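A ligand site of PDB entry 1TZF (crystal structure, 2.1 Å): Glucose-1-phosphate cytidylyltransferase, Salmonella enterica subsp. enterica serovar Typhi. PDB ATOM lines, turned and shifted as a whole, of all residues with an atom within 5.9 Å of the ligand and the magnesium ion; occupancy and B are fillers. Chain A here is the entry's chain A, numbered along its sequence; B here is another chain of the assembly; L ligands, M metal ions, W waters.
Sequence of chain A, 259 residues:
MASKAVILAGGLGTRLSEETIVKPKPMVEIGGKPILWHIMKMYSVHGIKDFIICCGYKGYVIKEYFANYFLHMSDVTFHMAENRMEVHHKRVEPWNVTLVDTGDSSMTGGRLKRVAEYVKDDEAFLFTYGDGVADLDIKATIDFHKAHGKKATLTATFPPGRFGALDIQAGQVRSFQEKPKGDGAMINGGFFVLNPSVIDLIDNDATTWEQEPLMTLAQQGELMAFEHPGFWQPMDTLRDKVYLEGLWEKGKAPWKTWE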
ATOM      1  N   LEU A   8       4.045 -28.142   7.005  1.00  0.00           N
ATOM      2  CA  LEU A   8       2.918 -29.046   6.949  1.00  0.00           C
ATOM      3  C   LEU A   8       1.745 -28.388   6.261  1.00  0.00           C
ATOM      4  O   LEU A   8       1.294 -27.319   6.662  1.00  0.00           O
ATOM      5  CB  LEU A   8       2.468 -29.479   8.351  1.00  0.00           C
ATOM      6  CG  LEU A   8       3.580 -30.232   9.061  1.00  0.00           C
ATOM      7  CD1 LEU A   8       3.265 -30.357  10.551  1.00  0.00           C
ATOM      8  CD2 LEU A   8       3.763 -31.617   8.449  1.00  0.00           C
ATOM      9  N   ALA A   9       1.266 -29.082   5.236  1.00  0.00           N
ATOM     10  CA  ALA A   9       0.138 -28.565   4.470  1.00  0.00           C
ATOM     11  C   ALA A   9      -0.835 -29.649   4.010  1.00  0.00           C
ATOM     12  O   ALA A   9      -1.585 -29.472   3.047  1.00  0.00           O
ATOM     13  CB  ALA A   9       0.599 -27.668   3.328  1.00  0.00           C
ATOM     14  N   GLY A  10      -0.830 -30.763   4.713  1.00  0.00           N
ATOM     15  CA  GLY A  10      -1.726 -31.872   4.409  1.00  0.00           C
ATOM     16  C   GLY A  10      -2.908 -31.814   5.365  1.00  0.00           C
ATOM     17  O   GLY A  10      -3.222 -30.761   5.950  1.00  0.00           O
ATOM     18  N   GLY A  11      -3.558 -32.970   5.541  1.00  0.00           N
ATOM     19  CA  GLY A  11      -4.714 -33.084   6.417  1.00  0.00           C
ATOM     20  C   GLY A  11      -6.042 -32.897   5.669  1.00  0.00           C
ATOM     21  O   GLY A  11      -6.170 -33.176   4.467  1.00  0.00           O
ATOM     22  N   LEU A  12      -7.008 -32.416   6.436  1.00  0.00           N
ATOM     23  CA  LEU A  12      -8.386 -32.140   6.100  1.00  0.00           C
ATOM     24  C   LEU A  12      -8.720 -31.193   4.937  1.00  0.00           C
ATOM     25  O   LEU A  12      -8.027 -30.230   4.574  1.00  0.00           O
ATOM     26  CB  LEU A  12      -9.161 -31.681   7.342  1.00  0.00           C
ATOM     27  CG  LEU A  12      -9.840 -32.831   8.068  1.00  0.00           C
ATOM     28  CD1 LEU A  12     -11.195 -32.336   8.569  1.00  0.00           C
ATOM     29  CD2 LEU A  12      -9.970 -34.023   7.120  1.00  0.00           C
ATOM     30  N   LYS A  25      -5.558 -26.163   3.859  1.00  0.00           N
ATOM     31  CA  LYS A  25      -5.626 -25.162   4.884  1.00  0.00           C
ATOM     32  C   LYS A  25      -4.664 -23.997   4.668  1.00  0.00           C
ATOM     33  O   LYS A  25      -5.035 -22.826   4.849  1.00  0.00           O
ATOM     34  CB  LYS A  25      -5.424 -25.798   6.241  1.00  0.00           C
ATOM     35  CG  LYS A  25      -6.212 -25.119   7.350  1.00  0.00           C
ATOM     36  CD  LYS A  25      -5.624 -25.392   8.725  1.00  0.00           C
ATOM     37  CE  LYS A  25      -6.310 -24.577   9.817  1.00  0.00           C
ATOM     38  NZ  LYS A  25      -6.726 -25.383  10.970  1.00  0.00           N
ATOM     39  N   PRO A  26      -3.422 -24.309   4.306  1.00  0.00           N
ATOM     40  CA  PRO A  26      -2.426 -23.260   4.131  1.00  0.00           C
ATOM     41  C   PRO A  26      -2.653 -22.327   2.946  1.00  0.00           C
ATOM     42  O   PRO A  26      -2.080 -21.214   2.824  1.00  0.00           O
ATOM     43  CB  PRO A  26      -1.060 -23.946   4.181  1.00  0.00           C
ATOM     44  CG  PRO A  26      -1.309 -25.263   4.916  1.00  0.00           C
ATOM     45  CD  PRO A  26      -2.795 -25.570   4.781  1.00  0.00           C
ATOM     46  N   CYS A  54       5.102 -30.154   2.697  1.00  0.00           N
ATOM     47  CA  CYS A  54       4.524 -31.473   2.819  1.00  0.00           C
ATOM     48  C   CYS A  54       3.099 -31.413   2.378  1.00  0.00           C
ATOM     49  O   CYS A  54       2.246 -30.987   3.164  1.00  0.00           O
ATOM     50  CB  CYS A  54       4.541 -31.991   4.243  1.00  0.00           C
ATOM     51  SG  CYS A  54       6.225 -32.138   4.873  1.00  0.00           S
ATOM     52  N   SER A 105      -3.475 -39.379   3.510  1.00  0.00           N
ATOM     53  CA  SER A 105      -3.763 -39.856   4.854  1.00  0.00           C
ATOM     54  C   SER A 105      -2.705 -39.673   5.946  1.00  0.00           C
ATOM     55  O   SER A 105      -2.994 -39.813   7.137  1.00  0.00           O
ATOM     56  CB  SER A 105      -4.262 -41.297   4.796  1.00  0.00           C
ATOM     57  OG  SER A 105      -5.607 -41.267   4.343  1.00  0.00           O
ATOM     58  N   SER A 106      -1.460 -39.395   5.578  1.00  0.00           N
ATOM     59  CA  SER A 106      -0.477 -39.265   6.619  1.00  0.00           C
ATOM     60  C   SER A 106      -0.796 -38.228   7.704  1.00  0.00           C
ATOM     61  O   SER A 106      -1.533 -37.249   7.539  1.00  0.00           O
ATOM     62  CB  SER A 106       0.963 -39.162   6.139  1.00  0.00           C
ATOM     63  OG  SER A 106       1.091 -39.586   4.801  1.00  0.00           O
ATOM     64  N   MET A 107      -0.188 -38.526   8.829  1.00  0.00           N
ATOM     65  CA  MET A 107      -0.221 -37.768  10.040  1.00  0.00           C
ATOM     66  C   MET A 107       0.975 -36.883   9.983  1.00  0.00           C
ATOM     67  O   MET A 107       1.839 -37.043   9.106  1.00  0.00           O
ATOM     68  CB  MET A 107      -0.149 -38.710  11.256  1.00  0.00           C
ATOM     69  CG  MET A 107      -1.455 -39.458  11.355  1.00  0.00           C
ATOM     70  SD  MET A 107      -2.839 -38.302  11.170  1.00  0.00           S
ATOM     71  CE  MET A 107      -4.226 -39.389  10.818  1.00  0.00           C
ATOM     72  N   THR A 108       1.008 -35.935  10.896  1.00  0.00           N
ATOM     73  CA  THR A 108       2.097 -34.984  10.921  1.00  0.00           C
ATOM     74  C   THR A 108       3.471 -35.554  11.031  1.00  0.00           C
ATOM     75  O   THR A 108       4.374 -35.047  10.347  1.00  0.00           O
ATOM     76  CB  THR A 108       1.892 -33.915  11.974  1.00  0.00           C
ATOM     77  OG1 THR A 108       1.765 -34.565  13.229  1.00  0.00           O
ATOM     78  CG2 THR A 108       0.623 -33.179  11.544  1.00  0.00           C
ATOM     79  N   ARG A 111       4.378 -37.244   7.638  1.00  0.00           N
ATOM     80  CA  ARG A 111       4.783 -36.303   6.602  1.00  0.00           C
ATOM     81  C   ARG A 111       6.236 -35.889   6.692  1.00  0.00           C
ATOM     82  O   ARG A 111       6.953 -35.774   5.688  1.00  0.00           O
ATOM     83  CB  ARG A 111       3.871 -35.080   6.591  1.00  0.00           C
ATOM     84  CG  ARG A 111       2.395 -35.462   6.555  1.00  0.00           C
ATOM     85  CD  ARG A 111       1.504 -34.325   6.078  1.00  0.00           C
ATOM     86  NE  ARG A 111       0.124 -34.774   6.065  1.00  0.00           N
ATOM     87  CZ  ARG A 111      -0.463 -35.166   4.976  1.00  0.00           C
ATOM     88  NH1 ARG A 111       0.190 -35.184   3.802  1.00  0.00           N
ATOM     89  NH2 ARG A 111      -1.717 -35.620   5.046  1.00  0.00           N
ATOM     90  N   TYR A 129       3.815 -25.668  11.352  1.00  0.00           N
ATOM     91  CA  TYR A 129       2.442 -25.789  10.899  1.00  0.00           C
ATOM     92  C   TYR A 129       2.190 -24.738   9.820  1.00  0.00           C
ATOM     93  O   TYR A 129       2.736 -23.625   9.904  1.00  0.00           O
ATOM     94  CB  TYR A 129       1.472 -25.531  12.088  1.00  0.00           C
ATOM     95  CG  TYR A 129       1.823 -26.466  13.245  1.00  0.00           C
ATOM     96  CD1 TYR A 129       2.406 -25.992  14.423  1.00  0.00           C
ATOM     97  CD2 TYR A 129       1.598 -27.833  13.125  1.00  0.00           C
ATOM     98  CE1 TYR A 129       2.733 -26.850  15.478  1.00  0.00           C
ATOM     99  CE2 TYR A 129       1.940 -28.724  14.155  1.00  0.00           C
ATOM    100  CZ  TYR A 129       2.514 -28.225  15.325  1.00  0.00           C
ATOM    101  OH  TYR A 129       2.842 -29.079  16.318  1.00  0.00           O
ATOM    102  N   GLY A 130       1.387 -25.060   8.783  1.00  0.00           N
ATOM    103  CA  GLY A 130       1.108 -24.105   7.703  1.00  0.00           C
ATOM    104  C   GLY A 130      -0.053 -23.151   8.007  1.00  0.00           C
ATOM    105  O   GLY A 130      -0.603 -22.493   7.105  1.00  0.00           O
ATOM    106  N   ASP A 131      -0.440 -23.059   9.273  1.00  0.00           N
ATOM    107  CA  ASP A 131      -1.549 -22.190   9.621  1.00  0.00           C
ATOM    108  C   ASP A 131      -1.288 -21.185  10.744  1.00  0.00           C
ATOM    109  O   ASP A 131      -2.232 -20.628  11.279  1.00  0.00           O
ATOM    110  CB  ASP A 131      -2.793 -23.048   9.922  1.00  0.00           C
ATOM    111  CG  ASP A 131      -2.598 -23.832  11.168  1.00  0.00           C
ATOM    112  OD1 ASP A 131      -1.520 -24.040  11.698  1.00  0.00           O
ATOM    113  OD2 ASP A 131      -3.711 -24.214  11.698  1.00  0.00           O
ATOM    114  N   ILE A 187       1.529 -22.607  25.032  1.00  0.00           N
ATOM    115  CA  ILE A 187       1.275 -23.869  24.384  1.00  0.00           C
ATOM    116  C   ILE A 187       2.225 -24.035  23.235  1.00  0.00           C
ATOM    117  O   ILE A 187       3.074 -23.158  23.064  1.00  0.00           O
ATOM    118  CB  ILE A 187      -0.157 -23.915  23.913  1.00  0.00           C
ATOM    119  CG1 ILE A 187      -0.502 -22.589  23.215  1.00  0.00           C
ATOM    120  CG2 ILE A 187      -1.016 -24.145  25.145  1.00  0.00           C
ATOM    121  CD1 ILE A 187       0.031 -22.446  21.772  1.00  0.00           C
ATOM    122  N   ASN A 188       2.052 -25.157  22.510  1.00  0.00           N
ATOM    123  CA  ASN A 188       2.859 -25.490  21.353  1.00  0.00           C
ATOM    124  C   ASN A 188       2.535 -24.559  20.202  1.00  0.00           C
ATOM    125  O   ASN A 188       1.501 -24.685  19.561  1.00  0.00           O
ATOM    126  CB  ASN A 188       2.691 -26.970  20.932  1.00  0.00           C
ATOM    127  CG  ASN A 188       3.386 -27.305  19.631  1.00  0.00           C
ATOM    128  OD1 ASN A 188       4.359 -26.636  19.227  1.00  0.00           O
ATOM    129  ND2 ASN A 188       2.878 -28.326  18.945  1.00  0.00           N
ATOM    130  N   GLY A 189       3.424 -23.610  19.962  1.00  0.00           N
ATOM    131  CA  GLY A 189       3.154 -22.708  18.878  1.00  0.00           C
ATOM    132  C   GLY A 189       3.806 -23.215  17.603  1.00  0.00           C
ATOM    133  O   GLY A 189       3.742 -22.567  16.593  1.00  0.00           O
ATOM    134  N   GLY A 190       4.460 -24.363  17.657  1.00  0.00           N
ATOM    135  CA  GLY A 190       5.109 -24.889  16.477  1.00  0.00           C
ATOM    136  C   GLY A 190       6.473 -24.275  16.308  1.00  0.00           C
ATOM    137  O   GLY A 190       7.278 -24.282  17.223  1.00  0.00           O
ATOM    138  N   GLU A 210       2.904 -34.823  17.353  1.00  0.00           N
ATOM    139  CA  GLU A 210       2.505 -34.355  18.653  1.00  0.00           C
ATOM    140  C   GLU A 210       2.207 -35.470  19.609  1.00  0.00           C
ATOM    141  O   GLU A 210       1.826 -35.264  20.758  1.00  0.00           O
ATOM    142  CB  GLU A 210       1.355 -33.373  18.560  1.00  0.00           C
ATOM    143  CG  GLU A 210       1.740 -32.217  17.631  1.00  0.00           C
ATOM    144  CD  GLU A 210       1.681 -32.616  16.169  1.00  0.00           C
ATOM    145  OE1 GLU A 210       1.123 -33.624  15.760  1.00  0.00           O
ATOM    146  OE2 GLU A 210       2.290 -31.759  15.395  1.00  0.00           O
ATOM    147  N   TRP A 232       1.406 -14.146  17.963  1.00  0.00           N
ATOM    148  CA  TRP A 232       1.248 -15.479  17.424  1.00  0.00           C
ATOM    149  C   TRP A 232      -0.221 -15.773  17.283  1.00  0.00           C
ATOM    150  O   TRP A 232      -0.988 -15.784  18.276  1.00  0.00           O
ATOM    151  CB  TRP A 232       1.903 -16.618  18.276  1.00  0.00           C
ATOM    152  CG  TRP A 232       1.591 -17.991  17.690  1.00  0.00           C
ATOM    153  CD1 TRP A 232       2.197 -18.584  16.620  1.00  0.00           C
ATOM    154  CD2 TRP A 232       0.565 -18.926  18.111  1.00  0.00           C
ATOM    155  NE1 TRP A 232       1.621 -19.796  16.335  1.00  0.00           N
ATOM    156  CE2 TRP A 232       0.620 -20.034  17.236  1.00  0.00           C
ATOM    157  CE3 TRP A 232      -0.384 -18.915  19.139  1.00  0.00           C
ATOM    158  CZ2 TRP A 232      -0.253 -21.122  17.367  1.00  0.00           C
ATOM    159  CZ3 TRP A 232      -1.221 -19.996  19.276  1.00  0.00           C
ATOM    160  CH2 TRP A 232      -1.170 -21.073  18.405  1.00  0.00           C
ATOM    161  N   PRO A 234      -2.928 -18.494  15.125  1.00  0.00           N
ATOM    162  CA  PRO A 234      -3.190 -19.635  14.270  1.00  0.00           C
ATOM    163  C   PRO A 234      -4.477 -19.306  13.546  1.00  0.00           C
ATOM    164  O   PRO A 234      -5.261 -18.506  14.063  1.00  0.00           O
ATOM    165  CB  PRO A 234      -3.547 -20.777  15.213  1.00  0.00           C
ATOM    166  CG  PRO A 234      -4.143 -20.089  16.444  1.00  0.00           C
ATOM    167  CD  PRO A 234      -3.575 -18.698  16.461  1.00  0.00           C
ATOM    168  N   MET A 235      -4.697 -19.884  12.359  1.00  0.00           N
ATOM    169  CA  MET A 235      -5.927 -19.593  11.620  1.00  0.00           C
ATOM    170  C   MET A 235      -6.760 -20.825  11.601  1.00  0.00           C
ATOM    171  O   MET A 235      -6.609 -21.648  10.690  1.00  0.00           O
ATOM    172  CB  MET A 235      -5.689 -19.109  10.185  1.00  0.00           C
ATOM    173  CG  MET A 235      -7.014 -18.642   9.572  1.00  0.00           C
ATOM    174  SD  MET A 235      -6.800 -17.802   7.993  1.00  0.00           S
ATOM    175  CE  MET A 235      -6.184 -19.174   6.989  1.00  0.00           C
ATOM    176  N   ASP A 236      -7.583 -20.970  12.632  1.00  0.00           N
ATOM    177  CA  ASP A 236      -8.387 -22.167  12.786  1.00  0.00           C
ATOM    178  C   ASP A 236      -9.855 -21.924  12.529  1.00  0.00           C
ATOM    179  O   ASP A 236     -10.580 -22.734  11.947  1.00  0.00           O
ATOM    180  CB  ASP A 236      -8.206 -22.661  14.244  1.00  0.00           C
ATOM    181  CG  ASP A 236      -6.868 -23.296  14.561  1.00  0.00           C
ATOM    182  OD1 ASP A 236      -6.253 -24.023  13.780  1.00  0.00           O
ATOM    183  OD2 ASP A 236      -6.439 -23.032  15.782  1.00  0.00           O
ATOM    184  N   ARG B 162      -7.309 -27.360  22.825  1.00  0.00           N
ATOM    185  CA  ARG B 162      -7.259 -27.088  21.389  1.00  0.00           C
ATOM    186  C   ARG B 162      -5.821 -27.059  20.878  1.00  0.00           C
ATOM    187  O   ARG B 162      -5.560 -27.035  19.679  1.00  0.00           O
ATOM    188  CB  ARG B 162      -8.034 -25.821  20.984  1.00  0.00           C
ATOM    189  CG  ARG B 162      -9.493 -25.754  21.450  1.00  0.00           C
ATOM    190  CD  ARG B 162     -10.400 -26.812  20.822  1.00  0.00           C
ATOM    191  NE  ARG B 162     -11.845 -26.584  21.010  1.00  0.00           N
ATOM    192  CZ  ARG B 162     -12.707 -27.587  21.172  1.00  0.00           C
ATOM    193  NH1 ARG B 162     -12.270 -28.844  21.188  1.00  0.00           N
ATOM    194  NH2 ARG B 162     -14.021 -27.332  21.314  1.00  0.00           N
ATOM    195  N   PHE B 163      -4.858 -27.057  21.812  1.00  0.00           N
ATOM    196  CA  PHE B 163      -3.466 -27.018  21.434  1.00  0.00           C
ATOM    197  C   PHE B 163      -2.656 -28.062  22.181  1.00  0.00           C
ATOM    198  O   PHE B 163      -3.177 -28.804  23.012  1.00  0.00           O
ATOM    199  CB  PHE B 163      -2.892 -25.606  21.684  1.00  0.00           C
ATOM    200  CG  PHE B 163      -3.692 -24.533  20.945  1.00  0.00           C
ATOM    201  CD1 PHE B 163      -4.705 -23.830  21.600  1.00  0.00           C
ATOM    202  CD2 PHE B 163      -3.467 -24.261  19.600  1.00  0.00           C
ATOM    203  CE1 PHE B 163      -5.478 -22.865  20.935  1.00  0.00           C
ATOM    204  CE2 PHE B 163      -4.228 -23.299  18.914  1.00  0.00           C
ATOM    205  CZ  PHE B 163      -5.245 -22.610  19.578  1.00  0.00           C
ATOM    206  N   GLY B 164      -1.361 -28.107  21.827  1.00  0.00           N
ATOM    207  CA  GLY B 164      -0.397 -29.001  22.466  1.00  0.00           C
ATOM    208  C   GLY B 164      -0.022 -28.381  23.827  1.00  0.00           C
ATOM    209  O   GLY B 164       0.577 -27.294  23.893  1.00  0.00           O
ATOM    210  N   ALA B 165      -0.405 -29.034  24.926  1.00  0.00           N
ATOM    211  CA  ALA B 165      -0.107 -28.527  26.273  1.00  0.00           C
ATOM    212  C   ALA B 165       1.348 -28.731  26.694  1.00  0.00           C
ATOM    213  O   ALA B 165       1.947 -29.783  26.422  1.00  0.00           O
ATOM    214  CB  ALA B 165      -1.001 -29.181  27.302  1.00  0.00           C
ATOM    215  N   PHE B 176       4.846 -33.024  27.435  1.00  0.00           N
ATOM    216  CA  PHE B 176       4.045 -32.579  26.306  1.00  0.00           C
ATOM    217  C   PHE B 176       2.793 -33.404  26.199  1.00  0.00           C
ATOM    218  O   PHE B 176       2.887 -34.627  26.232  1.00  0.00           O
ATOM    219  CB  PHE B 176       4.781 -32.741  24.954  1.00  0.00           C
ATOM    220  CG  PHE B 176       3.982 -32.163  23.795  1.00  0.00           C
ATOM    221  CD1 PHE B 176       4.241 -30.884  23.301  1.00  0.00           C
ATOM    222  CD2 PHE B 176       2.938 -32.871  23.194  1.00  0.00           C
ATOM    223  CE1 PHE B 176       3.508 -30.306  22.264  1.00  0.00           C
ATOM    224  CE2 PHE B 176       2.182 -32.311  22.150  1.00  0.00           C
ATOM    225  CZ  PHE B 176       2.473 -31.029  21.675  1.00  0.00           C
ATOM    226  N   GLU B 178      -0.874 -33.479  23.855  1.00  0.00           N
ATOM    227  CA  GLU B 178      -1.677 -32.957  22.774  1.00  0.00           C
ATOM    228  C   GLU B 178      -3.125 -32.829  23.197  1.00  0.00           C
ATOM    229  O   GLU B 178      -3.747 -33.832  23.549  1.00  0.00           O
ATOM    230  CB  GLU B 178      -1.558 -33.893  21.569  1.00  0.00           C
ATOM    231  CG  GLU B 178      -2.302 -33.364  20.341  1.00  0.00           C
ATOM    232  CD  GLU B 178      -1.941 -31.972  19.909  1.00  0.00           C
ATOM    233  OE1 GLU B 178      -2.560 -31.374  19.048  1.00  0.00           O
ATOM    234  OE2 GLU B 178      -0.913 -31.469  20.531  1.00  0.00           O
ATOM    235  N   LYS B 179      -3.648 -31.594  23.162  1.00  0.00           N
ATOM    236  CA  LYS B 179      -5.026 -31.265  23.491  1.00  0.00           C
ATOM    237  C   LYS B 179      -5.666 -32.052  24.642  1.00  0.00           C
ATOM    238  O   LYS B 179      -6.656 -32.791  24.496  1.00  0.00           O
ATOM    239  CB  LYS B 179      -5.913 -31.386  22.268  1.00  0.00           C
ATOM    240  CG  LYS B 179      -5.280 -30.883  20.996  1.00  0.00           C
ATOM    241  CD  LYS B 179      -6.368 -30.830  19.938  1.00  0.00           C
ATOM    242  CE  LYS B 179      -5.953 -30.076  18.699  1.00  0.00           C
ATOM    243  NZ  LYS B 179      -5.391 -30.993  17.703  1.00  0.00           N
HETATM  244  N1  LIG L   1      -1.425 -30.927   8.844  1.00  0.00           N
HETATM  245  C1  LIG L   1      -0.801 -31.862   8.041  1.00  0.00           C
HETATM  246  N2  LIG L   1      -1.280 -33.134   8.172  1.00  0.00           N
HETATM  247  C2  LIG L   1      -2.312 -33.570   9.005  1.00  0.00           C
HETATM  248  C3  LIG L   1      -2.906 -32.524   9.776  1.00  0.00           C
HETATM  249  C4  LIG L   1      -2.456 -31.290   9.684  1.00  0.00           C
HETATM  250  O1  LIG L   1       0.112 -31.610   7.240  1.00  0.00           O
HETATM  251  N3  LIG L   1      -2.620 -34.753   8.993  1.00  0.00           N
HETATM  252  C5  LIG L   1      -1.010 -29.527   8.772  1.00  0.00           C
HETATM  253  C6  LIG L   1      -2.160 -28.602   8.377  1.00  0.00           C
HETATM  254  O2  LIG L   1      -2.293 -28.454   6.963  1.00  0.00           O
HETATM  255  C7  LIG L   1      -1.821 -27.245   9.026  1.00  0.00           C
HETATM  256  C8  LIG L   1      -0.968 -27.693  10.209  1.00  0.00           C
HETATM  257  O3  LIG L   1      -0.579 -29.089  10.018  1.00  0.00           O
HETATM  258  O4  LIG L   1      -1.146 -26.330   8.162  1.00  0.00           O
HETATM  259  C9  LIG L   1      -1.666 -27.592  11.523  1.00  0.00           C
HETATM  260  O5  LIG L   1      -2.793 -28.487  11.470  1.00  0.00           O
HETATM  261  P1  LIG L   1      -4.095 -28.161  12.367  1.00  0.00           P
HETATM  262  O6  LIG L   1      -4.450 -26.718  12.445  1.00  0.00           O
HETATM  263  O7  LIG L   1      -5.281 -28.978  12.084  1.00  0.00           O
HETATM  264  O8  LIG L   1      -3.476 -28.638  13.810  1.00  0.00           O
HETATM  265  P2  LIG L   1      -3.904 -28.193  15.220  1.00  0.00           P
HETATM  266  O9  LIG L   1      -5.148 -28.895  15.666  1.00  0.00           O
HETATM  267  O10 LIG L   1      -4.207 -26.713  15.130  1.00  0.00           O
HETATM  268  O11 LIG L   1      -2.683 -28.502  16.258  1.00  0.00           O
HETATM  269  C10 LIG L   1      -1.360 -28.235  15.860  1.00  0.00           C
HETATM  270  C11 LIG L   1      -0.526 -29.026  16.854  1.00  0.00           C
HETATM  271  O12 LIG L   1      -1.008 -30.391  16.794  1.00  0.00           O
HETATM  272  C12 LIG L   1      -0.730 -28.462  18.276  1.00  0.00           C
HETATM  273  O13 LIG L   1       0.089 -29.114  19.251  1.00  0.00           O
HETATM  274  C13 LIG L   1      -0.399 -26.997  18.286  1.00  0.00           C
HETATM  275  O14 LIG L   1      -0.480 -26.431  19.594  1.00  0.00           O
HETATM  276  C14 LIG L   1      -1.266 -26.245  17.258  1.00  0.00           C
HETATM  277  C15 LIG L   1      -0.841 -24.802  17.136  1.00  0.00           C
HETATM  278  O15 LIG L   1      -1.683 -24.118  16.214  1.00  0.00           O
HETATM  279  O16 LIG L   1      -1.106 -26.804  15.929  1.00  0.00           O
HETATM  280 MG    MG M   1      -4.133 -25.217  13.625  1.00  0.00          MG
HETATM  281  O   HOH W   1      -0.318 -22.929  14.205  1.00  0.00           O
HETATM  282  O   HOH W   2      -5.670 -30.026   8.969  1.00  0.00           O
HETATM  283  O   HOH W   3      -3.692 -24.091  15.041  1.00  0.00           O
HETATM  284  O   HOH W   4      -6.529 -25.891  17.452  1.00  0.00           O
HETATM  285  O   HOH W   5      -5.196 -35.305  10.214  1.00  0.00           O
HETATM  286  O   HOH W   6      -2.205 -25.400  13.558  1.00  0.00           O
HETATM  287  O   HOH W   7      -4.744 -32.053  13.228  1.00  0.00           O
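Water W6 bridges OD1 of Asp 131 (2.4 Å) and O16 of the ligand (3.0 Å). Water W1 lies within hydrogen-bond range of an oxygen (O15) of the ligand and the side-chain carboxylate of Asp 131. Water W4 lies within hydrogen-bond range of O of Arg 162 of chain B (2.7 Å) and OD2 of Asp 236 (3.3 Å).
Water W3 is bound to the magnesium ion. The magnesium ion is bound by an oxygen (O6) of the ligand, 1.9 Å away. Water W6 is bound to the magnesium ion, 1.9 Å away. An oxygen (O10) of the ligand is bound to the magnesium ion (2.1 Å). OD2 of Asp 131 is bound to the magnesium ion (2.2 Å). OD1 of Asp 236 is bound to the magnesium ion.
Merely in contact with the magnesium ion: Lys 25 (3.7 Å). The nearest printed residue that does not touch the magnesium ion is Pro 234 (4.8 Å).
OD2 of Asp 131 lies close to NZ of Lys 25 (3.3 Å). The backbone NH (N) of Met 235 is in hydrogen-bond range of the backbone carbonyl oxygen (O) of Asp 131, 2.8 Å away. O of Cys 54 is in hydrogen-bond range of N of Gly 10, 3.5 Å away. The side-chain carboxylate (OE1) of Glu 178 of chain B lies within salt-bridge range of the side-chain amino group (NZ) of Lys 179 of chain B (3.2 Å). The guanidinium group (NH2) of Arg 111 sits at hydrogen-bond distance from the backbone carbonyl oxygen (O) of Ser 106, at 3.0 Å. The side-chain carboxylate of Glu 210 lies within hydrogen-bond range of the side-chain hydroxyl of Tyr 129. The side-chain carboxylate (OE1) of Glu 210 lies within hydrogen-bond range of the side-chain hydroxyl (OG1) of Thr 108 (2.8 Å). NE1 of Trp 232 sits at hydrogen-bond distance from O of Gly 189 (3.5 Å).
O of Asn 188 is in hydrogen-bond range of O14 of the ligand (2.6 Å). The side-chain amide nitrogen of Asn 188 sits at hydrogen-bond distance from an oxygen (O13) of the ligand (2.9 Å). N of Gly 10 sits at hydrogen-bond distance from O1 of the ligand (2.8 Å). The backbone carbonyl oxygen (O) of Gly 10 sits at hydrogen-bond distance from an oxygen (O2) of the ligand (2.7 Å). OE2 of Glu 178 of chain B lies within hydrogen-bond range of O13 of the ligand. An oxygen (O4) of the ligand lies within hydrogen-bond range of the backbone NH (N) of Gly 130, 2.9 Å away. N of Gly 164 of chain B lies within hydrogen-bond range of O14 of the ligand, 2.9 Å away. O9 of the ligand is in salt-bridge range of NZ of Lys 179 of chain B (2.9 Å). The guanidinium group (NE) of Arg 111 is in hydrogen-bond range of a nitrogen (N2) of the ligand. NZ of Lys 25 lies close to O6 of the ligand, 3.0 Å away. O4 of the ligand sits at hydrogen-bond distance from O of Leu 8 (3.0 Å). A nitrogen (N3) of the ligand lies within hydrogen-bond range of the backbone carbonyl oxygen of Ser 106 (3.1 Å). N of Ala 9 sits at hydrogen-bond distance from O1 of the ligand (3.4 Å). N of Gly 11 lies within hydrogen-bond range of N2 of the ligand (3.5 Å).
CG of Pro 26 touches O4 of the ligand (3.4 Å). Met 107 touches the ligand (CA to N3, 3.99 Å). Thr 108 touches the ligand. OH of Tyr 129 touches C11 of the ligand (3.4 Å). CG of Glu 210 touches O12 of the ligand, 3.4 Å away. Trp 232 touches the ligand (CZ2 to O15, 3.5 Å). CB of Pro 234 touches O15 of the ligand, at 3.95 Å. CB of Phe 163 of chain B touches O14 of the ligand, at 3.3 Å. Phe 176 of chain B touches the ligand (CZ to O13, 3.9 Å). Hydrophobic or aromatic side chains within 4 Å of the ligand: Leu 8, Pro 26, Tyr 129, Trp 232, Pro 234, Phe 163 of chain B and Phe 176 of chain B.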
